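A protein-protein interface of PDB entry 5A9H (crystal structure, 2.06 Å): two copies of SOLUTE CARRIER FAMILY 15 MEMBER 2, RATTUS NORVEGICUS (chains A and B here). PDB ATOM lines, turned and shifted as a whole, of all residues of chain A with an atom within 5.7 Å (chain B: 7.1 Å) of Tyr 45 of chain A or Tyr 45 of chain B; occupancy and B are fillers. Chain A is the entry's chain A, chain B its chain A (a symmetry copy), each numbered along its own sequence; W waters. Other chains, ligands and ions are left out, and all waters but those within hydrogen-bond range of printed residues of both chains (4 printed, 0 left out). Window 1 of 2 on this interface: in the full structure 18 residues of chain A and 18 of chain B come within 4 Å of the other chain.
Water W4 lies within hydrogen-bond range of the backbone carbonyl oxygen (O) of Asp 193 of chain B (2.8 Å), the backbone NH (N) of Thr 173 of chain B (2.9 Å) and the side-chain amino group (NZ) of Lys 47 of chain A (3.2 Å). Water W2 bridges O of Lys 47 of chain B and OG1 of Thr 43 of chain A.
Tyr 45 of chain A touches its own counterpart, Tyr 45 of chain B. Tyr 45 of chain A touches Lys 47 of chain B, and with the chains exchanged Lys 47 of chain A touches Tyr 45 of chain B. Positions printed for both chains: 8, 9, 10, 42, 43, 44, 45, 46, 47, 192, 193 and 194.
Of the 12 printed residues of chain A, 9 touch a printed residue of chain B. Hydrophobic or aromatic side chains of chain B that line the printed part of chain A: Phe 8, Leu 32, His 44, Tyr 45 and Ile 194. Among the printed residues, 20 pairs touch across the chains. Among the printed residues, no Asp or Glu carboxylate lies within 4 Å of a Lys or Arg side-chain nitrogen of the other chain.
Of the printed residues of chain B, Tyr 45 of chain A touches His 44, Tyr 45 and Lys 47. Of the printed residues of chain B, Glu 192 of chain A touches Glu 6. Printed residues of chain B within 4 Å of Thr 43 of chain A: Ser 46 (3.3 Å) and Lys 47 (2.8 Å). Asn 41 of chain B touches none of the printed residues of chain A. The nearest printed residue of chain B that does not touch Tyr 45 of chain A is Phe 8 of chain B (4.1 Å). The nearest printed residue of chain A that does not touch Tyr 45 of chain B is Phe 8 of chain A (4.1 Å).
The backbone carbonyl oxygen (O) of Glu 192 of chain A is in hydrogen-bond range of the side-chain amide nitrogen (NE2) of Gln 10 of chain A (3.1 Å). O of Phe 8 of chain B lies within hydrogen-bond range of N of Tyr 80 of chain B (3.0 Å). N of Leu 9 of chain B sits at hydrogen-bond distance from O of Ser 46 of chain B (2.8 Å).
N of Lys 47 of chain B is in hydrogen-bond range of O of Thr 43 of chain A (2.8 Å). ND1 of His 44 of chain A lies within hydrogen-bond range of OE2 of Glu 34 of chain B, 3.4 Å away. A ring nitrogen (ND1) of His 44 of chain A is in hydrogen-bond range of the side-chain hydroxyl (OG) of Ser 46 of chain B (3.1 Å). The backbone NH (N) of Tyr 45 of chain A lies within hydrogen-bond range of the backbone carbonyl oxygen (O) of Tyr 45 of chain B, at 2.8 Å. OG of Ser 46 of chain A lies within hydrogen-bond range of ND1 of His 44 of chain B, 3.1 Å away. O of Thr 43 of chain B sits at hydrogen-bond distance from N of Lys 47 of chain A, 2.8 Å away. The backbone carbonyl oxygen (O) of Asp 193 of chain B lies within hydrogen-bond range of the side-chain amino group (NZ) of Lys 47 of chain A. The side-chain amino group of Lys 47 of chain B lies within hydrogen-bond range of the backbone carbonyl oxygen of Asp 193 of chain A. The side-chain carboxylate of Glu 6 of chain B sits close to the side-chain carboxylate of Glu 192 of chain A, at 3.4 Å.
Among the printed residues, pairs that only touch across the chains: Phe 8 of chain A with Ile 194 of chain B (3.7 Å), Thr 43 of chain A with Ser 46 of chain B (3.3 Å), His 44 of chain A with Leu 32 of chain B (3.3 Å), His 44 of chain A with Tyr 45 of chain B (3.3 Å), Tyr 45 of chain A with His 44 of chain B (3.3 Å), Tyr 45 of chain A with Lys 47 of chain B (3.4 Å), Ser 46 of chain A with Thr 43 of chain B (3.3 Å), Lys 47 of chain A with Tyr 45 of chain B (3.4 Å), Lys 47 of chain A with Ile 194 of chain B (3.3 Å), Ile 194 of chain A with Phe 8 of chain B (3.7 Å) and Ile 194 of chain A with Lys 47 of chain B (3.3 Å).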
ATOM      1  N   PHE A   8      11.723 -17.062  -3.416  1.00  0.00           N
ATOM      2  CA  PHE A   8      11.283 -15.760  -2.946  1.00  0.00           C
ATOM      3  C   PHE A   8      11.138 -15.861  -1.442  1.00  0.00           C
ATOM      4  O   PHE A   8      10.752 -16.907  -0.922  1.00  0.00           O
ATOM      5  CB  PHE A   8       9.974 -15.305  -3.568  1.00  0.00           C
ATOM      6  CG  PHE A   8      10.164 -14.661  -4.912  1.00  0.00           C
ATOM      7  CD1 PHE A   8      10.614 -13.345  -5.016  1.00  0.00           C
ATOM      8  CD2 PHE A   8       9.922 -15.374  -6.082  1.00  0.00           C
ATOM      9  CE1 PHE A   8      10.772 -12.741  -6.263  1.00  0.00           C
ATOM     10  CE2 PHE A   8      10.088 -14.770  -7.329  1.00  0.00           C
ATOM     11  CZ  PHE A   8      10.508 -13.454  -7.411  1.00  0.00           C
ATOM     12  N   LEU A   9      11.483 -14.780  -0.748  1.00  0.00           N
ATOM     13  CA  LEU A   9      11.376 -14.706   0.701  1.00  0.00           C
ATOM     14  C   LEU A   9      10.764 -13.381   1.117  1.00  0.00           C
ATOM     15  O   LEU A   9      11.127 -12.312   0.607  1.00  0.00           O
ATOM     16  CB  LEU A   9      12.740 -14.925   1.394  1.00  0.00           C
ATOM     17  CG  LEU A   9      12.751 -14.847   2.961  1.00  0.00           C
ATOM     18  CD1 LEU A   9      12.058 -16.064   3.585  1.00  0.00           C
ATOM     19  CD2 LEU A   9      14.168 -14.770   3.494  1.00  0.00           C
ATOM     20  N   GLN A  10       9.835 -13.469   2.053  1.00  0.00           N
ATOM     21  CA  GLN A  10       9.215 -12.314   2.699  1.00  0.00           C
ATOM     22  C   GLN A  10       9.527 -12.447   4.183  1.00  0.00           C
ATOM     23  O   GLN A  10       9.268 -13.486   4.807  1.00  0.00           O
ATOM     24  CB  GLN A  10       7.688 -12.284   2.468  1.00  0.00           C
ATOM     25  CG  GLN A  10       6.939 -11.113   3.154  1.00  0.00           C
ATOM     26  CD  GLN A  10       5.489 -11.163   2.772  1.00  0.00           C
ATOM     27  OE1 GLN A  10       4.985 -12.170   2.235  1.00  0.00           O
ATOM     28  NE2 GLN A  10       4.804 -10.066   2.950  1.00  0.00           N
ATOM     29  N   THR A  42       4.977  -6.148   5.088  1.00  0.00           N
ATOM     30  CA  THR A  42       3.691  -6.665   4.584  1.00  0.00           C
ATOM     31  C   THR A  42       3.704  -6.876   3.056  1.00  0.00           C
ATOM     32  O   THR A  42       2.951  -7.730   2.570  1.00  0.00           O
ATOM     33  CB  THR A  42       2.519  -5.740   4.938  1.00  0.00           C
ATOM     34  OG1 THR A  42       2.733  -4.494   4.299  1.00  0.00           O
ATOM     35  CG2 THR A  42       2.318  -5.555   6.445  1.00  0.00           C
ATOM     36  N   THR A  43       4.495  -6.055   2.291  1.00  0.00           N
ATOM     37  CA  THR A  43       4.501  -6.130   0.807  1.00  0.00           C
ATOM     38  C   THR A  43       5.863  -5.952   0.143  1.00  0.00           C
ATOM     39  O   THR A  43       5.937  -5.352  -0.941  1.00  0.00           O
ATOM     40  CB  THR A  43       3.501  -5.121   0.190  1.00  0.00           C
ATOM     41  OG1 THR A  43       3.794  -3.827   0.712  1.00  0.00           O
ATOM     42  CG2 THR A  43       2.044  -5.478   0.439  1.00  0.00           C
ATOM     43  N   HIS A  44       6.934  -6.430   0.783  1.00  0.00           N
ATOM     44  CA  HIS A  44       8.305  -6.359   0.261  1.00  0.00           C
ATOM     45  C   HIS A  44       8.863  -7.778   0.279  1.00  0.00           C
ATOM     46  O   HIS A  44       8.636  -8.526   1.236  1.00  0.00           O
ATOM     47  CB  HIS A  44       9.192  -5.405   1.089  1.00  0.00           C
ATOM     48  CG  HIS A  44       8.802  -3.960   1.010  1.00  0.00           C
ATOM     49  ND1 HIS A  44       9.747  -2.970   0.900  1.00  0.00           N
ATOM     50  CD2 HIS A  44       7.578  -3.388   1.040  1.00  0.00           C
ATOM     51  CE1 HIS A  44       9.081  -1.832   0.919  1.00  0.00           C
ATOM     52  NE2 HIS A  44       7.771  -2.036   0.986  1.00  0.00           N
ATOM     53  N   TYR A  45       9.542  -8.158  -0.803  1.00  0.00           N
ATOM     54  CA  TYR A  45      10.040  -9.509  -1.048  1.00  0.00           C
ATOM     55  C   TYR A  45      11.443  -9.503  -1.625  1.00  0.00           C
ATOM     56  O   TYR A  45      11.826  -8.571  -2.328  1.00  0.00           O
ATOM     57  CB  TYR A  45       9.093 -10.193  -2.090  1.00  0.00           C
ATOM     58  CG  TYR A  45       7.610  -9.957  -1.825  1.00  0.00           C
ATOM     59  CD1 TYR A  45       6.905 -10.759  -0.931  1.00  0.00           C
ATOM     60  CD2 TYR A  45       6.934  -8.892  -2.418  1.00  0.00           C
ATOM     61  CE1 TYR A  45       5.566 -10.500  -0.624  1.00  0.00           C
ATOM     62  CE2 TYR A  45       5.607  -8.608  -2.098  1.00  0.00           C
ATOM     63  CZ  TYR A  45       4.923  -9.422  -1.207  1.00  0.00           C
ATOM     64  OH  TYR A  45       3.609  -9.179  -0.902  1.00  0.00           O
ATOM     65  N   SER A  46      12.179 -10.577  -1.381  1.00  0.00           N
ATOM     66  CA  SER A  46      13.518 -10.727  -1.912  1.00  0.00           C
ATOM     67  C   SER A  46      13.663 -12.043  -2.639  1.00  0.00           C
ATOM     68  O   SER A  46      12.974 -13.025  -2.318  1.00  0.00           O
ATOM     69  CB  SER A  46      14.548 -10.629  -0.798  1.00  0.00           C
ATOM     70  OG  SER A  46      14.418  -9.357  -0.186  1.00  0.00           O
ATOM     71  N   LYS A  47      14.569 -12.049  -3.622  1.00  0.00           N
ATOM     72  CA  LYS A  47      14.906 -13.243  -4.366  1.00  0.00           C
ATOM     73  C   LYS A  47      16.251 -13.737  -3.831  1.00  0.00           C
ATOM     74  O   LYS A  47      17.185 -12.952  -3.682  1.00  0.00           O
ATOM     75  CB  LYS A  47      15.012 -12.933  -5.863  1.00  0.00           C
ATOM     76  CG  LYS A  47      14.169 -13.865  -6.702  1.00  0.00           C
ATOM     77  CD  LYS A  47      14.541 -13.800  -8.168  1.00  0.00           C
ATOM     78  CE  LYS A  47      13.827 -12.726  -8.940  1.00  0.00           C
ATOM     79  NZ  LYS A  47      14.043 -12.908 -10.402  1.00  0.00           N
ATOM     80  N   GLU A 192       0.684  -9.688   3.006  1.00  0.00           N
ATOM     81  CA  GLU A 192       0.263 -10.195   1.706  1.00  0.00           C
ATOM     82  C   GLU A 192       1.320 -11.105   1.124  1.00  0.00           C
ATOM     83  O   GLU A 192       2.496 -10.725   1.057  1.00  0.00           O
ATOM     84  CB  GLU A 192      -0.003  -9.041   0.732  1.00  0.00           C
ATOM     85  CG  GLU A 192      -1.159  -8.161   1.151  1.00  0.00           C
ATOM     86  CD  GLU A 192      -1.431  -6.976   0.249  1.00  0.00           C
ATOM     87  OE1 GLU A 192      -1.300  -7.116  -0.992  1.00  0.00           O
ATOM     88  OE2 GLU A 192      -1.802  -5.909   0.790  1.00  0.00           O
ATOM     89  N   ASP A 193       0.893 -12.292   0.651  1.00  0.00           N
ATOM     90  CA  ASP A 193       1.798 -13.246  -0.012  1.00  0.00           C
ATOM     91  C   ASP A 193       2.185 -12.618  -1.356  1.00  0.00           C
ATOM     92  O   ASP A 193       1.363 -11.914  -1.941  1.00  0.00           O
ATOM     93  CB  ASP A 193       1.087 -14.563  -0.295  1.00  0.00           C
ATOM     94  CG  ASP A 193       0.766 -15.426   0.912  1.00  0.00           C
ATOM     95  OD1 ASP A 193       0.682 -14.879   2.028  1.00  0.00           O
ATOM     96  OD2 ASP A 193       0.525 -16.642   0.723  1.00  0.00           O
ATOM     97  N   ILE A 194       3.411 -12.863  -1.842  1.00  0.00           N
ATOM     98  CA  ILE A 194       3.896 -12.310  -3.105  1.00  0.00           C
ATOM     99  C   ILE A 194       2.941 -12.517  -4.306  1.00  0.00           C
ATOM    100  O   ILE A 194       2.431 -13.610  -4.489  1.00  0.00           O
ATOM    101  CB  ILE A 194       5.320 -12.823  -3.421  1.00  0.00           C
ATOM    102  CG1 ILE A 194       5.905 -12.032  -4.602  1.00  0.00           C
ATOM    103  CG2 ILE A 194       5.332 -14.371  -3.605  1.00  0.00           C
ATOM    104  CD1 ILE A 194       7.375 -12.082  -4.778  1.00  0.00           C
ATOM    105  N   GLU B   6      -2.699  -3.771  -8.950  1.00  0.00           N
ATOM    106  CA  GLU B   6      -1.408  -3.955  -8.251  1.00  0.00           C
ATOM    107  C   GLU B   6      -0.264  -3.944  -9.260  1.00  0.00           C
ATOM    108  O   GLU B   6      -0.423  -4.424 -10.393  1.00  0.00           O
ATOM    109  CB  GLU B   6      -1.317  -5.317  -7.531  1.00  0.00           C
ATOM    110  CG  GLU B   6      -2.205  -5.517  -6.328  1.00  0.00           C
ATOM    111  CD  GLU B   6      -1.694  -6.606  -5.404  1.00  0.00           C
ATOM    112  OE1 GLU B   6      -1.655  -7.787  -5.819  1.00  0.00           O
ATOM    113  OE2 GLU B   6      -1.307  -6.273  -4.264  1.00  0.00           O
ATOM    114  N   PHE B   8       4.366  -4.484  -9.325  1.00  0.00           N
ATOM    115  CA  PHE B   8       5.617  -4.772  -8.646  1.00  0.00           C
ATOM    116  C   PHE B   8       6.576  -3.654  -8.996  1.00  0.00           C
ATOM    117  O   PHE B   8       6.543  -3.131 -10.110  1.00  0.00           O
ATOM    118  CB  PHE B   8       6.218  -6.114  -9.029  1.00  0.00           C
ATOM    119  CG  PHE B   8       5.629  -7.255  -8.249  1.00  0.00           C
ATOM    120  CD1 PHE B   8       6.031  -7.506  -6.937  1.00  0.00           C
ATOM    121  CD2 PHE B   8       4.651  -8.070  -8.809  1.00  0.00           C
ATOM    122  CE1 PHE B   8       5.501  -8.577  -6.219  1.00  0.00           C
ATOM    123  CE2 PHE B   8       4.115  -9.136  -8.086  1.00  0.00           C
ATOM    124  CZ  PHE B   8       4.548  -9.386  -6.796  1.00  0.00           C
ATOM    125  N   LEU B   9       7.403  -3.268  -8.029  1.00  0.00           N
ATOM    126  CA  LEU B   9       8.402  -2.227  -8.214  1.00  0.00           C
ATOM    127  C   LEU B   9       9.729  -2.657  -7.617  1.00  0.00           C
ATOM    128  O   LEU B   9       9.793  -3.192  -6.502  1.00  0.00           O
ATOM    129  CB  LEU B   9       7.944  -0.874  -7.623  1.00  0.00           C
ATOM    130  CG  LEU B   9       8.952   0.323  -7.745  1.00  0.00           C
ATOM    131  CD1 LEU B   9       9.063   0.812  -9.195  1.00  0.00           C
ATOM    132  CD2 LEU B   9       8.527   1.486  -6.873  1.00  0.00           C
ATOM    133  N   GLN B  10      10.784  -2.412  -8.374  1.00  0.00           N
ATOM    134  CA  GLN B  10      12.165  -2.615  -7.942  1.00  0.00           C
ATOM    135  C   GLN B  10      12.837  -1.252  -8.032  1.00  0.00           C
ATOM    136  O   GLN B  10      12.800  -0.581  -9.074  1.00  0.00           O
ATOM    137  CB  GLN B  10      12.897  -3.639  -8.837  1.00  0.00           C
ATOM    138  CG  GLN B  10      14.385  -3.886  -8.477  1.00  0.00           C
ATOM    139  CD  GLN B  10      14.936  -4.960  -9.368  1.00  0.00           C
ATOM    140  OE1 GLN B  10      14.336  -5.334 -10.396  1.00  0.00           O
ATOM    141  NE2 GLN B  10      16.032  -5.544  -8.963  1.00  0.00           N
ATOM    142  N   VAL B  11      13.455  -0.854  -6.937  1.00  0.00           N
ATOM    143  CA  VAL B  11      14.153   0.415  -6.886  1.00  0.00           C
ATOM    144  C   VAL B  11      15.641   0.215  -7.034  1.00  0.00           C
ATOM    145  O   VAL B  11      16.255  -0.508  -6.266  1.00  0.00           O
ATOM    146  CB  VAL B  11      13.792   1.240  -5.635  1.00  0.00           C
ATOM    147  CG1 VAL B  11      14.518   2.581  -5.686  1.00  0.00           C
ATOM    148  CG2 VAL B  11      12.275   1.448  -5.550  1.00  0.00           C
ATOM    149  N   LEU B  32       4.380   3.076  -0.834  1.00  0.00           N
ATOM    150  CA  LEU B  32       5.694   2.517  -0.577  1.00  0.00           C
ATOM    151  C   LEU B  32       6.518   3.530   0.179  1.00  0.00           C
ATOM    152  O   LEU B  32       6.478   4.707  -0.158  1.00  0.00           O
ATOM    153  CB  LEU B  32       6.402   2.182  -1.921  1.00  0.00           C
ATOM    154  CG  LEU B  32       7.891   1.686  -1.823  1.00  0.00           C
ATOM    155  CD1 LEU B  32       7.948   0.268  -1.319  1.00  0.00           C
ATOM    156  CD2 LEU B  32       8.584   1.711  -3.165  1.00  0.00           C
ATOM    157  N   GLU B  34      10.509   3.472   1.437  1.00  0.00           N
ATOM    158  CA  GLU B  34      11.714   2.656   1.289  1.00  0.00           C
ATOM    159  C   GLU B  34      13.034   3.456   1.414  1.00  0.00           C
ATOM    160  O   GLU B  34      13.149   4.539   0.857  1.00  0.00           O
ATOM    161  CB  GLU B  34      11.617   2.026  -0.116  1.00  0.00           C
ATOM    162  CG  GLU B  34      12.691   1.039  -0.511  1.00  0.00           C
ATOM    163  CD  GLU B  34      12.351  -0.382  -0.147  1.00  0.00           C
ATOM    164  OE1 GLU B  34      12.624  -0.774   1.008  1.00  0.00           O
ATOM    165  OE2 GLU B  34      11.786  -1.092  -1.004  1.00  0.00           O
ATOM    166  N   ASN B  41      18.521  -1.764  -5.250  1.00  0.00           N
ATOM    167  CA  ASN B  41      18.300  -3.170  -4.844  1.00  0.00           C
ATOM    168  C   ASN B  41      18.417  -4.104  -6.062  1.00  0.00           C
ATOM    169  O   ASN B  41      17.584  -4.006  -6.970  1.00  0.00           O
ATOM    170  CB  ASN B  41      16.897  -3.305  -4.245  1.00  0.00           C
ATOM    171  CG  ASN B  41      16.664  -2.553  -2.945  1.00  0.00           C
ATOM    172  OD1 ASN B  41      17.503  -2.555  -2.043  1.00  0.00           O
ATOM    173  ND2 ASN B  41      15.477  -1.975  -2.787  1.00  0.00           N
ATOM    174  N   THR B  42      19.403  -5.029  -6.079  1.00  0.00           N
ATOM    175  CA  THR B  42      19.532  -5.959  -7.215  1.00  0.00           C
ATOM    176  C   THR B  42      18.462  -7.070  -7.185  1.00  0.00           C
ATOM    177  O   THR B  42      18.117  -7.589  -8.255  1.00  0.00           O
ATOM    178  CB  THR B  42      20.917  -6.618  -7.268  1.00  0.00           C
ATOM    179  OG1 THR B  42      21.081  -7.390  -6.091  1.00  0.00           O
ATOM    180  CG2 THR B  42      22.065  -5.618  -7.431  1.00  0.00           C
ATOM    181  N   THR B  43      17.992  -7.489  -5.966  1.00  0.00           N
ATOM    182  CA  THR B  43      17.027  -8.613  -5.840  1.00  0.00           C
ATOM    183  C   THR B  43      15.947  -8.439  -4.777  1.00  0.00           C
ATOM    184  O   THR B  43      15.561  -9.428  -4.134  1.00  0.00           O
ATOM    185  CB  THR B  43      17.760  -9.957  -5.602  1.00  0.00           C
ATOM    186  OG1 THR B  43      18.626  -9.801  -4.481  1.00  0.00           O
ATOM    187  CG2 THR B  43      18.539 -10.448  -6.812  1.00  0.00           C
ATOM    188  N   HIS B  44      15.479  -7.206  -4.561  1.00  0.00           N
ATOM    189  CA  HIS B  44      14.424  -6.883  -3.593  1.00  0.00           C
ATOM    190  C   HIS B  44      13.344  -6.116  -4.350  1.00  0.00           C
ATOM    191  O   HIS B  44      13.656  -5.262  -5.186  1.00  0.00           O
ATOM    192  CB  HIS B  44      14.959  -6.057  -2.404  1.00  0.00           C
ATOM    193  CG  HIS B  44      15.920  -6.789  -1.516  1.00  0.00           C
ATOM    194  ND1 HIS B  44      15.862  -6.670  -0.149  1.00  0.00           N
ATOM    195  CD2 HIS B  44      16.940  -7.615  -1.835  1.00  0.00           C
ATOM    196  CE1 HIS B  44      16.871  -7.378   0.318  1.00  0.00           C
ATOM    197  NE2 HIS B  44      17.538  -7.978  -0.660  1.00  0.00           N
ATOM    198  N   TYR B  45      12.083  -6.464  -4.092  1.00  0.00           N
ATOM    199  CA  TYR B  45      10.912  -5.954  -4.801  1.00  0.00           C
ATOM    200  C   TYR B  45       9.769  -5.637  -3.856  1.00  0.00           C
ATOM    201  O   TYR B  45       9.627  -6.266  -2.811  1.00  0.00           O
ATOM    202  CB  TYR B  45      10.425  -7.064  -5.791  1.00  0.00           C
ATOM    203  CG  TYR B  45      11.553  -7.745  -6.560  1.00  0.00           C
ATOM    204  CD1 TYR B  45      12.065  -7.183  -7.727  1.00  0.00           C
ATOM    205  CD2 TYR B  45      12.148  -8.910  -6.080  1.00  0.00           C
ATOM    206  CE1 TYR B  45      13.151  -7.761  -8.393  1.00  0.00           C
ATOM    207  CE2 TYR B  45      13.249  -9.477  -6.722  1.00  0.00           C
ATOM    208  CZ  TYR B  45      13.741  -8.904  -7.886  1.00  0.00           C
ATOM    209  OH  TYR B  45      14.802  -9.464  -8.549  1.00  0.00           O
ATOM    210  N   SER B  46       8.919  -4.705  -4.263  1.00  0.00           N
ATOM    211  CA  SER B  46       7.754  -4.338  -3.484  1.00  0.00           C
ATOM    212  C   SER B  46       6.502  -4.406  -4.326  1.00  0.00           C
ATOM    213  O   SER B  46       6.551  -4.224  -5.554  1.00  0.00           O
ATOM    214  CB  SER B  46       7.918  -2.941  -2.905  1.00  0.00           C
ATOM    215  OG  SER B  46       9.067  -2.939  -2.074  1.00  0.00           O
ATOM    216  N   LYS B  47       5.379  -4.671  -3.649  1.00  0.00           N
ATOM    217  CA  LYS B  47       4.075  -4.686  -4.276  1.00  0.00           C
ATOM    218  C   LYS B  47       3.380  -3.379  -3.891  1.00  0.00           C
ATOM    219  O   LYS B  47       3.376  -3.001  -2.721  1.00  0.00           O
ATOM    220  CB  LYS B  47       3.257  -5.886  -3.788  1.00  0.00           C
ATOM    221  CG  LYS B  47       2.702  -6.704  -4.931  1.00  0.00           C
ATOM    222  CD  LYS B  47       1.620  -7.657  -4.473  1.00  0.00           C
ATOM    223  CE  LYS B  47       2.130  -8.985  -3.988  1.00  0.00           C
ATOM    224  NZ  LYS B  47       1.003  -9.944  -3.819  1.00  0.00           N
ATOM    225  N   LEU B  48       2.843  -2.672  -4.887  1.00  0.00           N
ATOM    226  CA  LEU B  48       2.127  -1.413  -4.706  1.00  0.00           C
ATOM    227  C   LEU B  48       0.673  -1.585  -5.117  1.00  0.00           C
ATOM    228  O   LEU B  48       0.398  -2.161  -6.172  1.00  0.00           O
ATOM    229  CB  LEU B  48       2.762  -0.278  -5.543  1.00  0.00           C
ATOM    230  CG  LEU B  48       3.983   0.429  -4.899  1.00  0.00           C
ATOM    231  CD1 LEU B  48       5.223  -0.470  -4.885  1.00  0.00           C
ATOM    232  CD2 LEU B  48       4.330   1.723  -5.623  1.00  0.00           C
ATOM    233  N   TYR B  80       7.869  -3.055 -12.748  1.00  0.00           N
ATOM    234  CA  TYR B  80       8.665  -1.889 -13.116  1.00  0.00           C
ATOM    235  C   TYR B  80       9.967  -1.790 -12.326  1.00  0.00           C
ATOM    236  O   TYR B  80      10.080  -2.315 -11.227  1.00  0.00           O
ATOM    237  CB  TYR B  80       7.855  -0.602 -12.866  1.00  0.00           C
ATOM    238  CG  TYR B  80       6.585  -0.483 -13.692  1.00  0.00           C
ATOM    239  CD1 TYR B  80       6.599   0.121 -14.944  1.00  0.00           C
ATOM    240  CD2 TYR B  80       5.369  -0.950 -13.206  1.00  0.00           C
ATOM    241  CE1 TYR B  80       5.439   0.232 -15.708  1.00  0.00           C
ATOM    242  CE2 TYR B  80       4.197  -0.822 -13.951  1.00  0.00           C
ATOM    243  CZ  TYR B  80       4.241  -0.255 -15.213  1.00  0.00           C
ATOM    244  OH  TYR B  80       3.090  -0.123 -15.952  1.00  0.00           O
ATOM    245  N   GLN B  81      10.953  -1.104 -12.902  1.00  0.00           N
ATOM    246  CA  GLN B  81      12.201  -0.797 -12.223  1.00  0.00           C
ATOM    247  C   GLN B  81      12.326   0.705 -12.233  1.00  0.00           C
ATOM    248  O   GLN B  81      12.178   1.330 -13.284  1.00  0.00           O
ATOM    249  CB  GLN B  81      13.419  -1.457 -12.890  1.00  0.00           C
ATOM    250  CG  GLN B  81      13.466  -2.971 -12.648  1.00  0.00           C
ATOM    251  CD  GLN B  81      14.293  -3.703 -13.681  1.00  0.00           C
ATOM    252  OE1 GLN B  81      14.264  -3.385 -14.867  1.00  0.00           O
ATOM    253  NE2 GLN B  81      15.058  -4.701 -13.259  1.00  0.00           N
ATOM    254  N   ASP B  98       9.117  -3.946 -17.079  1.00  0.00           N
ATOM    255  CA  ASP B  98       9.772  -5.234 -17.334  1.00  0.00           C
ATOM    256  C   ASP B  98       8.933  -6.217 -18.179  1.00  0.00           C
ATOM    257  O   ASP B  98       7.706  -6.193 -18.082  1.00  0.00           O
ATOM    258  CB  ASP B  98      10.142  -5.914 -16.013  1.00  0.00           C
ATOM    259  CG  ASP B  98      11.192  -5.177 -15.190  1.00  0.00           C
ATOM    260  OD1 ASP B  98      11.664  -4.089 -15.643  1.00  0.00           O
ATOM    261  OD2 ASP B  98      11.540  -5.674 -14.105  1.00  0.00           O
ATOM    262  N   THR B 173      16.253 -13.129 -15.878  1.00  0.00           N
ATOM    263  CA  THR B 173      16.275 -11.947 -16.730  1.00  0.00           C
ATOM    264  C   THR B 173      17.051 -10.856 -15.978  1.00  0.00           C
ATOM    265  O   THR B 173      16.793 -10.591 -14.801  1.00  0.00           O
ATOM    266  CB  THR B 173      14.843 -11.551 -17.110  1.00  0.00           C
ATOM    267  OG1 THR B 173      14.269 -12.635 -17.827  1.00  0.00           O
ATOM    268  CG2 THR B 173      14.800 -10.306 -17.970  1.00  0.00           C
ATOM    269  N   ALA B 191      21.503  -5.987 -12.237  1.00  0.00           N
ATOM    270  CA  ALA B 191      20.302  -6.144 -11.426  1.00  0.00           C
ATOM    271  C   ALA B 191      19.458  -7.262 -12.037  1.00  0.00           C
ATOM    272  O   ALA B 191      19.604  -7.593 -13.219  1.00  0.00           O
ATOM    273  CB  ALA B 191      19.520  -4.837 -11.356  1.00  0.00           C
ATOM    274  N   GLU B 192      18.592  -7.873 -11.231  1.00  0.00           N
ATOM    275  CA  GLU B 192      17.746  -8.951 -11.727  1.00  0.00           C
ATOM    276  C   GLU B 192      16.292  -8.537 -11.707  1.00  0.00           C
ATOM    277  O   GLU B 192      15.797  -8.065 -10.675  1.00  0.00           O
ATOM    278  CB  GLU B 192      17.923 -10.216 -10.879  1.00  0.00           C
ATOM    279  CG  GLU B 192      19.315 -10.801 -10.964  1.00  0.00           C
ATOM    280  CD  GLU B 192      19.556 -12.024 -10.104  1.00  0.00           C
ATOM    281  OE1 GLU B 192      18.637 -12.870  -9.981  1.00  0.00           O
ATOM    282  OE2 GLU B 192      20.684 -12.144  -9.572  1.00  0.00           O
ATOM    283  N   ASP B 193      15.590  -8.762 -12.834  1.00  0.00           N
ATOM    284  CA  ASP B 193      14.148  -8.480 -12.932  1.00  0.00           C
ATOM    285  C   ASP B 193      13.441  -9.508 -12.043  1.00  0.00           C
ATOM    286  O   ASP B 193      13.926 -10.633 -11.935  1.00  0.00           O
ATOM    287  CB  ASP B 193      13.653  -8.672 -14.360  1.00  0.00           C
ATOM    288  CG  ASP B 193      14.109  -7.639 -15.375  1.00  0.00           C
ATOM    289  OD1 ASP B 193      15.148  -6.993 -15.138  1.00  0.00           O
ATOM    290  OD2 ASP B 193      13.463  -7.534 -16.443  1.00  0.00           O
ATOM    291  N   ILE B 194      12.316  -9.137 -11.413  1.00  0.00           N
ATOM    292  CA  ILE B 194      11.563 -10.025 -10.530  1.00  0.00           C
ATOM    293  C   ILE B 194      11.242 -11.414 -11.136  1.00  0.00           C
ATOM    294  O   ILE B 194      10.818 -11.489 -12.278  1.00  0.00           O
ATOM    295  CB  ILE B 194      10.285  -9.329 -10.007  1.00  0.00           C
ATOM    296  CG1 ILE B 194       9.656 -10.175  -8.887  1.00  0.00           C
ATOM    297  CG2 ILE B 194       9.317  -8.977 -11.178  1.00  0.00           C
ATOM    298  CD1 ILE B 194       8.693  -9.492  -7.994  1.00  0.00           C
HETATM  299  O   HOH W   1      -1.253 -11.992  -2.980  1.00  0.00           O
HETATM  300  O   HOH W   2       4.834  -1.334  -0.975  1.00  0.00           O
HETATM  301  O   HOH W   3      18.359 -11.327  -1.698  1.00  0.00           O
HETATM  302  O   HOH W   4      14.711 -12.845 -13.490  1.00  0.00           O
